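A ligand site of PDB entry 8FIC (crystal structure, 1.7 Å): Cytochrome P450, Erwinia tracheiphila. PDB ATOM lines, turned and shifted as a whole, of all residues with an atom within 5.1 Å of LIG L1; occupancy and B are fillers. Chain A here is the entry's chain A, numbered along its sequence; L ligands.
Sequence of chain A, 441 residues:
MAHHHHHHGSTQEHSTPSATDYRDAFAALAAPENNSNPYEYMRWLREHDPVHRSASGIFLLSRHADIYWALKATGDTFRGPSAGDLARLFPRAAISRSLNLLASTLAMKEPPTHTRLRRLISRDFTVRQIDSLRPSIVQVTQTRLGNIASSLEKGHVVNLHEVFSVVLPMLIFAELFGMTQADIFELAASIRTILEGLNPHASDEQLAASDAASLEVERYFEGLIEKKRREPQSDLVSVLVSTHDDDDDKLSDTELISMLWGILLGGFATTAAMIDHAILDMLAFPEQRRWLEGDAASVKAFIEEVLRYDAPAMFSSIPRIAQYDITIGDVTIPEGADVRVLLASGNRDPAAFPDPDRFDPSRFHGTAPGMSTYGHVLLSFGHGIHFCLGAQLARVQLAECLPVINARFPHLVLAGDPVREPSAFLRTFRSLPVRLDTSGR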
ATOM      1  N   LEU A 102      -7.017 -11.616   7.554  1.00  0.00           N
ATOM      2  CA  LEU A 102      -7.708 -10.334   7.437  1.00  0.00           C
ATOM      3  C   LEU A 102      -8.528 -10.257   6.160  1.00  0.00           C
ATOM      4  O   LEU A 102      -9.616  -9.652   6.151  1.00  0.00           O
ATOM      5  CB  LEU A 102      -6.685  -9.193   7.463  1.00  0.00           C
ATOM      6  CG  LEU A 102      -7.260  -7.768   7.463  1.00  0.00           C
ATOM      7  CD1 LEU A 102      -7.984  -7.480   8.772  1.00  0.00           C
ATOM      8  CD2 LEU A 102      -6.151  -6.740   7.210  1.00  0.00           C
ATOM      9  N   THR A 105     -12.164 -11.254   6.559  1.00  0.00           N
ATOM     10  CA  THR A 105     -13.037 -10.645   7.561  1.00  0.00           C
ATOM     11  C   THR A 105     -14.075  -9.779   6.864  1.00  0.00           C
ATOM     12  O   THR A 105     -13.859  -9.275   5.760  1.00  0.00           O
ATOM     13  CB  THR A 105     -12.267  -9.794   8.579  1.00  0.00           C
ATOM     14  OG1 THR A 105     -11.652  -8.678   7.925  1.00  0.00           O
ATOM     15  CG2 THR A 105     -11.206 -10.619   9.293  1.00  0.00           C
ATOM     16  N   LEU A 106     -15.214  -9.592   7.537  1.00  0.00           N
ATOM     17  CA  LEU A 106     -16.311  -8.846   6.943  1.00  0.00           C
ATOM     18  C   LEU A 106     -15.953  -7.390   6.717  1.00  0.00           C
ATOM     19  O   LEU A 106     -16.614  -6.713   5.916  1.00  0.00           O
ATOM     20  CB  LEU A 106     -17.563  -8.957   7.810  1.00  0.00           C
ATOM     21  CG  LEU A 106     -17.677  -8.062   9.044  1.00  0.00           C
ATOM     22  CD1 LEU A 106     -19.098  -8.093   9.594  1.00  0.00           C
ATOM     23  CD2 LEU A 106     -16.686  -8.472  10.137  1.00  0.00           C
ATOM     24  N   ALA A 107     -14.936  -6.865   7.405  1.00  0.00           N
ATOM     25  CA  ALA A 107     -14.520  -5.484   7.191  1.00  0.00           C
ATOM     26  C   ALA A 107     -13.909  -5.267   5.814  1.00  0.00           C
ATOM     27  O   ALA A 107     -13.777  -4.113   5.388  1.00  0.00           O
ATOM     28  CB  ALA A 107     -13.523  -5.052   8.270  1.00  0.00           C
ATOM     29  N   LEU A 195      -2.120  -7.402  16.347  1.00  0.00           N
ATOM     30  CA  LEU A 195      -2.671  -6.084  16.048  1.00  0.00           C
ATOM     31  C   LEU A 195      -1.626  -5.169  15.423  1.00  0.00           C
ATOM     32  O   LEU A 195      -1.875  -4.501  14.421  1.00  0.00           O
ATOM     33  CB  LEU A 195      -3.255  -5.453  17.312  1.00  0.00           C
ATOM     34  CG  LEU A 195      -4.586  -6.044  17.802  1.00  0.00           C
ATOM     35  CD1 LEU A 195      -4.953  -5.493  19.173  1.00  0.00           C
ATOM     36  CD2 LEU A 195      -5.709  -5.754  16.821  1.00  0.00           C
ATOM     37  N   LEU A 198      -0.819  -5.210  11.653  1.00  0.00           N
ATOM     38  CA  LEU A 198      -1.873  -4.860  10.698  1.00  0.00           C
ATOM     39  C   LEU A 198      -1.823  -3.383  10.333  1.00  0.00           C
ATOM     40  O   LEU A 198      -2.782  -2.634  10.508  1.00  0.00           O
ATOM     41  CB  LEU A 198      -3.235  -5.233  11.261  1.00  0.00           C
ATOM     42  CG  LEU A 198      -3.511  -6.712  11.552  1.00  0.00           C
ATOM     43  CD1 LEU A 198      -4.874  -6.869  12.209  1.00  0.00           C
ATOM     44  CD2 LEU A 198      -3.422  -7.527  10.275  1.00  0.00           C
ATOM     45  N   MET A 259     -13.483 -14.777  11.028  1.00  0.00           N
ATOM     46  CA  MET A 259     -14.415 -14.136  11.942  1.00  0.00           C
ATOM     47  C   MET A 259     -13.970 -14.323  13.394  1.00  0.00           C
ATOM     48  O   MET A 259     -14.006 -13.372  14.191  1.00  0.00           O
ATOM     49  CB  MET A 259     -15.821 -14.700  11.744  1.00  0.00           C
ATOM     50  CG  MET A 259     -16.888 -14.044  12.596  1.00  0.00           C
ATOM     51  SD  MET A 259     -17.308 -12.382  12.033  1.00  0.00           S
ATOM     52  CE  MET A 259     -18.266 -12.748  10.572  1.00  0.00           C
ATOM     53  N   TRP A 261     -10.885 -15.035  14.543  1.00  0.00           N
ATOM     54  CA  TRP A 261      -9.659 -14.260  14.678  1.00  0.00           C
ATOM     55  C   TRP A 261      -9.962 -12.761  14.752  1.00  0.00           C
ATOM     56  O   TRP A 261      -9.469 -12.061  15.654  1.00  0.00           O
ATOM     57  CB  TRP A 261      -8.747 -14.610  13.502  1.00  0.00           C
ATOM     58  CG  TRP A 261      -7.460 -13.879  13.345  1.00  0.00           C
ATOM     59  CD1 TRP A 261      -6.246 -14.201  13.906  1.00  0.00           C
ATOM     60  CD2 TRP A 261      -7.227 -12.735  12.518  1.00  0.00           C
ATOM     61  NE1 TRP A 261      -5.289 -13.310  13.484  1.00  0.00           N
ATOM     62  CE2 TRP A 261      -5.868 -12.402  12.635  1.00  0.00           C
ATOM     63  CE3 TRP A 261      -8.053 -11.947  11.700  1.00  0.00           C
ATOM     64  CZ2 TRP A 261      -5.304 -11.314  11.969  1.00  0.00           C
ATOM     65  CZ3 TRP A 261      -7.497 -10.869  11.039  1.00  0.00           C
ATOM     66  CH2 TRP A 261      -6.132 -10.559  11.174  1.00  0.00           C
ATOM     67  N   GLY A 262     -10.780 -12.253  13.837  1.00  0.00           N
ATOM     68  CA  GLY A 262     -10.986 -10.815  13.756  1.00  0.00           C
ATOM     69  C   GLY A 262     -11.739 -10.251  14.938  1.00  0.00           C
ATOM     70  O   GLY A 262     -11.383  -9.187  15.471  1.00  0.00           O
ATOM     71  N   ILE A 263     -12.802 -10.927  15.365  1.00  0.00           N
ATOM     72  CA  ILE A 263     -13.564 -10.442  16.515  1.00  0.00           C
ATOM     73  C   ILE A 263     -12.704 -10.461  17.776  1.00  0.00           C
ATOM     74  O   ILE A 263     -12.798  -9.570  18.616  1.00  0.00           O
ATOM     75  CB  ILE A 263     -14.864 -11.251  16.671  1.00  0.00           C
ATOM     76  CG1 ILE A 263     -15.781 -10.961  15.477  1.00  0.00           C
ATOM     77  CG2 ILE A 263     -15.553 -10.903  17.995  1.00  0.00           C
ATOM     78  CD1 ILE A 263     -17.037 -11.811  15.443  1.00  0.00           C
ATOM     79  N   LEU A 265      -9.487  -9.914  17.866  1.00  0.00           N
ATOM     80  CA  LEU A 265      -8.618  -8.747  17.772  1.00  0.00           C
ATOM     81  C   LEU A 265      -9.369  -7.477  18.140  1.00  0.00           C
ATOM     82  O   LEU A 265      -8.798  -6.564  18.751  1.00  0.00           O
ATOM     83  CB  LEU A 265      -8.044  -8.617  16.362  1.00  0.00           C
ATOM     84  CG  LEU A 265      -7.066  -9.676  15.859  1.00  0.00           C
ATOM     85  CD1 LEU A 265      -6.513  -9.220  14.509  1.00  0.00           C
ATOM     86  CD2 LEU A 265      -5.945  -9.925  16.860  1.00  0.00           C
ATOM     87  N   GLY A 266     -10.634  -7.380  17.746  1.00  0.00           N
ATOM     88  CA  GLY A 266     -11.386  -6.185  18.064  1.00  0.00           C
ATOM     89  C   GLY A 266     -12.022  -6.178  19.432  1.00  0.00           C
ATOM     90  O   GLY A 266     -12.523  -5.137  19.872  1.00  0.00           O
ATOM     91  N   THR A 270      -9.016  -2.097  22.076  1.00  0.00           N
ATOM     92  CA  THR A 270      -9.427  -0.710  21.894  1.00  0.00           C
ATOM     93  C   THR A 270     -10.304  -0.220  23.038  1.00  0.00           C
ATOM     94  O   THR A 270     -10.281   0.962  23.382  1.00  0.00           O
ATOM     95  CB  THR A 270     -10.169  -0.538  20.578  1.00  0.00           C
ATOM     96  OG1 THR A 270     -11.073  -1.631  20.398  1.00  0.00           O
ATOM     97  CG2 THR A 270      -9.197  -0.464  19.415  1.00  0.00           C
ATOM     98  N   ALA A 313      -7.634   3.934  17.643  1.00  0.00           N
ATOM     99  CA  ALA A 313      -7.002   3.623  16.364  1.00  0.00           C
ATOM    100  C   ALA A 313      -6.941   4.921  15.570  1.00  0.00           C
ATOM    101  O   ALA A 313      -7.979   5.423  15.132  1.00  0.00           O
ATOM    102  CB  ALA A 313      -7.777   2.537  15.622  1.00  0.00           C
ATOM    103  N   PHE A 315      -5.761   5.573  12.617  1.00  0.00           N
ATOM    104  CA  PHE A 315      -6.357   5.209  11.340  1.00  0.00           C
ATOM    105  C   PHE A 315      -6.633   3.714  11.379  1.00  0.00           C
ATOM    106  O   PHE A 315      -6.148   2.990  12.262  1.00  0.00           O
ATOM    107  CB  PHE A 315      -5.456   5.584  10.161  1.00  0.00           C
ATOM    108  CG  PHE A 315      -4.125   4.882  10.141  1.00  0.00           C
ATOM    109  CD1 PHE A 315      -3.980   3.657   9.508  1.00  0.00           C
ATOM    110  CD2 PHE A 315      -3.023   5.459  10.739  1.00  0.00           C
ATOM    111  CE1 PHE A 315      -2.756   3.013   9.488  1.00  0.00           C
ATOM    112  CE2 PHE A 315      -1.794   4.824  10.723  1.00  0.00           C
ATOM    113  CZ  PHE A 315      -1.658   3.603  10.088  1.00  0.00           C
ATOM    114  N   SER A 316      -7.442   3.241  10.438  1.00  0.00           N
ATOM    115  CA  SER A 316      -7.864   1.840  10.418  1.00  0.00           C
ATOM    116  C   SER A 316      -6.958   0.993   9.533  1.00  0.00           C
ATOM    117  O   SER A 316      -6.498   1.425   8.481  1.00  0.00           O
ATOM    118  CB  SER A 316      -9.314   1.728   9.924  1.00  0.00           C
ATOM    119  OG  SER A 316      -9.661   0.370   9.702  1.00  0.00           O
ATOM    120  N   SER A 317      -6.717  -0.243   9.986  1.00  0.00           N
ATOM    121  CA  SER A 317      -5.961  -1.233   9.233  1.00  0.00           C
ATOM    122  C   SER A 317      -6.664  -1.672   7.958  1.00  0.00           C
ATOM    123  O   SER A 317      -6.028  -2.310   7.108  1.00  0.00           O
ATOM    124  CB  SER A 317      -5.714  -2.475  10.098  1.00  0.00           C
ATOM    125  OG  SER A 317      -5.267  -2.135  11.395  1.00  0.00           O
ATOM    126  N   ILE A 318      -7.948  -1.379   7.820  1.00  0.00           N
ATOM    127  CA  ILE A 318      -8.748  -1.869   6.706  1.00  0.00           C
ATOM    128  C   ILE A 318      -8.483  -1.000   5.478  1.00  0.00           C
ATOM    129  O   ILE A 318      -8.747   0.205   5.506  1.00  0.00           O
ATOM    130  CB  ILE A 318     -10.246  -1.877   7.041  1.00  0.00           C
ATOM    131  CG1 ILE A 318     -10.524  -2.702   8.297  1.00  0.00           C
ATOM    132  CG2 ILE A 318     -11.049  -2.410   5.861  1.00  0.00           C
ATOM    133  CD1 ILE A 318      -9.969  -4.128   8.269  1.00  0.00           C
ATOM    134  N   PHE A 425      -0.131   2.861  14.743  1.00  0.00           N
ATOM    135  CA  PHE A 425      -1.500   3.333  14.577  1.00  0.00           C
ATOM    136  C   PHE A 425      -2.421   3.185  15.793  1.00  0.00           C
ATOM    137  O   PHE A 425      -3.445   3.851  15.841  1.00  0.00           O
ATOM    138  CB  PHE A 425      -2.174   2.623  13.387  1.00  0.00           C
ATOM    139  CG  PHE A 425      -2.536   1.169  13.644  1.00  0.00           C
ATOM    140  CD1 PHE A 425      -1.554   0.234  13.885  1.00  0.00           C
ATOM    141  CD2 PHE A 425      -3.862   0.754  13.594  1.00  0.00           C
ATOM    142  CE1 PHE A 425      -1.879  -1.100  14.097  1.00  0.00           C
ATOM    143  CE2 PHE A 425      -4.192  -0.588  13.802  1.00  0.00           C
ATOM    144  CZ  PHE A 425      -3.197  -1.498  14.054  1.00  0.00           C
ATOM    145  N   LEU A 426      -2.074   2.341  16.764  1.00  0.00           N
ATOM    146  CA  LEU A 426      -2.918   2.169  17.935  1.00  0.00           C
ATOM    147  C   LEU A 426      -2.430   3.048  19.082  1.00  0.00           C
ATOM    148  O   LEU A 426      -1.269   3.462  19.121  1.00  0.00           O
ATOM    149  CB  LEU A 426      -2.924   0.703  18.361  1.00  0.00           C
ATOM    150  CG  LEU A 426      -3.635  -0.234  17.384  1.00  0.00           C
ATOM    151  CD1 LEU A 426      -3.334  -1.685  17.688  1.00  0.00           C
ATOM    152  CD2 LEU A 426      -5.133   0.037  17.431  1.00  0.00           C
HETATM  153  C1  LIG L   1     -11.850  -5.341  13.363  1.00  0.00           C
HETATM  154  C2  LIG L   1     -10.464  -7.267  11.752  1.00  0.00           C
HETATM  155  C3  LIG L   1     -12.066  -5.419  11.837  1.00  0.00           C
HETATM  156  C4  LIG L   1     -13.431  -8.627  12.544  1.00  0.00           C
HETATM  157  C5  LIG L   1      -9.048  -1.047  12.902  1.00  0.00           C
HETATM  158  C6  LIG L   1      -8.118  -4.483  14.268  1.00  0.00           C
HETATM  159  C7  LIG L   1      -7.241  -3.223  14.318  1.00  0.00           C
HETATM  160  C8  LIG L   1      -7.952  -2.041  14.959  1.00  0.00           C
HETATM  161  C9  LIG L   1      -9.292  -1.729  14.268  1.00  0.00           C
HETATM  162  C10 LIG L   1     -10.128  -3.027  14.255  1.00  0.00           C
HETATM  163  C11 LIG L   1     -11.551  -2.847  13.699  1.00  0.00           C
HETATM  164  C12 LIG L   1     -12.407  -4.062  13.948  1.00  0.00           C
HETATM  165  C13 LIG L   1     -10.373  -5.508  13.733  1.00  0.00           C
HETATM  166  C14 LIG L   1      -9.797  -6.750  13.034  1.00  0.00           C
HETATM  167  C15 LIG L   1     -11.917  -6.913  11.573  1.00  0.00           C
HETATM  168  C16 LIG L   1     -12.765  -7.480  12.648  1.00  0.00           C
HETATM  169  C17 LIG L   1     -12.649  -6.589  13.849  1.00  0.00           C
HETATM  170  C18 LIG L   1      -9.984  -0.640  15.077  1.00  0.00           C
HETATM  171  C19 LIG L   1      -9.189  -3.970  12.051  1.00  0.00           C
HETATM  172  C20 LIG L   1      -9.458  -4.240  13.539  1.00  0.00           C
HETATM  173  O1  LIG L   1     -10.044  -0.830  12.161  1.00  0.00           O
HETATM  174  O2  LIG L   1      -7.878  -0.736  12.596  1.00  0.00           O
HETATM  175  C1  LG2 L   2     -15.379  -1.833  13.155  1.00  0.00           C
HETATM  176  C2  LG2 L   2     -13.104   0.973  16.409  1.00  0.00           C
HETATM  177  C3  LG2 L   2     -14.618  -1.898  19.986  1.00  0.00           C
HETATM  178  C4  LG2 L   2     -15.876  -5.182  16.651  1.00  0.00           C
HETATM  179  C5  LG2 L   2     -14.650  -0.799  13.706  1.00  0.00           C
HETATM  180  C6  LG2 L   2     -14.049   0.320  13.005  1.00  0.00           C
HETATM  181  C7  LG2 L   2     -13.427   1.077  13.920  1.00  0.00           C
HETATM  182  C8  LG2 L   2     -13.601   0.469  15.218  1.00  0.00           C
HETATM  183  C9  LG2 L   2     -12.656   2.382  13.654  1.00  0.00           C
HETATM  184  C10 LG2 L   2     -14.153   0.592  11.481  1.00  0.00           C
HETATM  185  C11 LG2 L   2     -12.926   0.123  10.726  1.00  0.00           C
HETATM  186  C12 LG2 L   2     -12.973   0.649   9.304  1.00  0.00           C
HETATM  187  O1  LG2 L   2     -14.067   1.078   8.851  1.00  0.00           O
HETATM  188  O2  LG2 L   2     -11.904   0.636   8.627  1.00  0.00           O
HETATM  189  C13 LG2 L   2     -13.410   0.504  17.664  1.00  0.00           C
HETATM  190  C14 LG2 L   2     -13.217   1.193  18.929  1.00  0.00           C
HETATM  191  C15 LG2 L   2     -13.632   0.397  19.919  1.00  0.00           C
HETATM  192  C16 LG2 L   2     -14.109  -0.824  19.309  1.00  0.00           C
HETATM  193  C17 LG2 L   2     -12.627   2.615  19.084  1.00  0.00           C
HETATM  194  C18 LG2 L   2     -13.665   0.649  21.447  1.00  0.00           C
HETATM  195  C19 LG2 L   2     -13.599   1.859  21.984  1.00  0.00           C
HETATM  196  C20 LG2 L   2     -15.075  -3.058  19.408  1.00  0.00           C
HETATM  197  C21 LG2 L   2     -15.528  -4.225  20.114  1.00  0.00           C
HETATM  198  C22 LG2 L   2     -15.869  -5.157  19.218  1.00  0.00           C
HETATM  199  C23 LG2 L   2     -15.658  -4.593  17.889  1.00  0.00           C
HETATM  200  C24 LG2 L   2     -15.582  -4.344  21.655  1.00  0.00           C
HETATM  201  C25 LG2 L   2     -16.411  -6.551  19.624  1.00  0.00           C
HETATM  202  C26 LG2 L   2     -16.625  -7.540  18.757  1.00  0.00           C
HETATM  203  C27 LG2 L   2     -15.867  -4.549  15.423  1.00  0.00           C
HETATM  204  C28 LG2 L   2     -16.225  -5.158  14.156  1.00  0.00           C
HETATM  205  C29 LG2 L   2     -16.099  -4.247  13.184  1.00  0.00           C
HETATM  206  C30 LG2 L   2     -15.654  -3.021  13.795  1.00  0.00           C
HETATM  207  C31 LG2 L   2     -16.679  -6.619  13.971  1.00  0.00           C
HETATM  208  C32 LG2 L   2     -16.375  -4.472  11.679  1.00  0.00           C
HETATM  209  C33 LG2 L   2     -17.828  -4.135  11.367  1.00  0.00           C
HETATM  210  C34 LG2 L   2     -18.158  -4.321   9.897  1.00  0.00           C
HETATM  211  O3  LG2 L   2     -17.227  -4.410   9.060  1.00  0.00           O
HETATM  212  O4  LG2 L   2     -19.376  -4.360   9.562  1.00  0.00           O
HETATM  213  N1  LG2 L   2     -14.348  -0.676  15.044  1.00  0.00           N
HETATM  214  N2  LG2 L   2     -13.953  -0.738  17.945  1.00  0.00           N
HETATM  215  N3  LG2 L   2     -15.170  -3.313  18.052  1.00  0.00           N
HETATM  216  N4  LG2 L   2     -15.519  -3.231  15.161  1.00  0.00           N
HETATM  217 FE1  LG2 L   2     -15.031  -1.869  16.607  1.00  0.00          FE
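The side-chain hydroxyl (OG) of Ser 316 lies within hydrogen-bond range of an oxygen (O1) of LIG L1 (2.8 Å). An oxygen (O2) of LIG L1 sits at hydrogen-bond distance from the backbone NH of Ser 317. OG of Ser 317 lies within hydrogen-bond range of O2 of LIG L1, 3.2 Å away. An oxygen (O2) of LG2 L2 lies within hydrogen-bond range of the side-chain hydroxyl (OG) of Ser 316 (2.5 Å).
OG of Ser 316 lies within hydrogen-bond range of N of Ile 318. The side-chain hydroxyl (OG) of Ser 317 lies within hydrogen-bond range of the backbone carbonyl oxygen (O) of Leu 198, 2.7 Å away. O of Leu 102 lies within hydrogen-bond range of OG1 of Thr 105 (2.9 Å).
CD1 of Leu 102 touches C2 of LIG L1 (3.9 Å). Ala 107 touches LIG L1 (CB to C3, 3.9 Å). Leu 195 touches LIG L1 (CD2 to C6, 3.7 Å). Gly 262 touches LIG L1. Ile 263 touches LIG L1. CB of Ala 313 touches C18 of LIG L1, at 3.9 Å. CD1 of Ile 318 touches C19 of LIG L1, 3.9 Å away. Phe 425 touches LIG L1. The nearest printed residue that does not touch LIG L1 is Leu 106 (4.1 Å).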
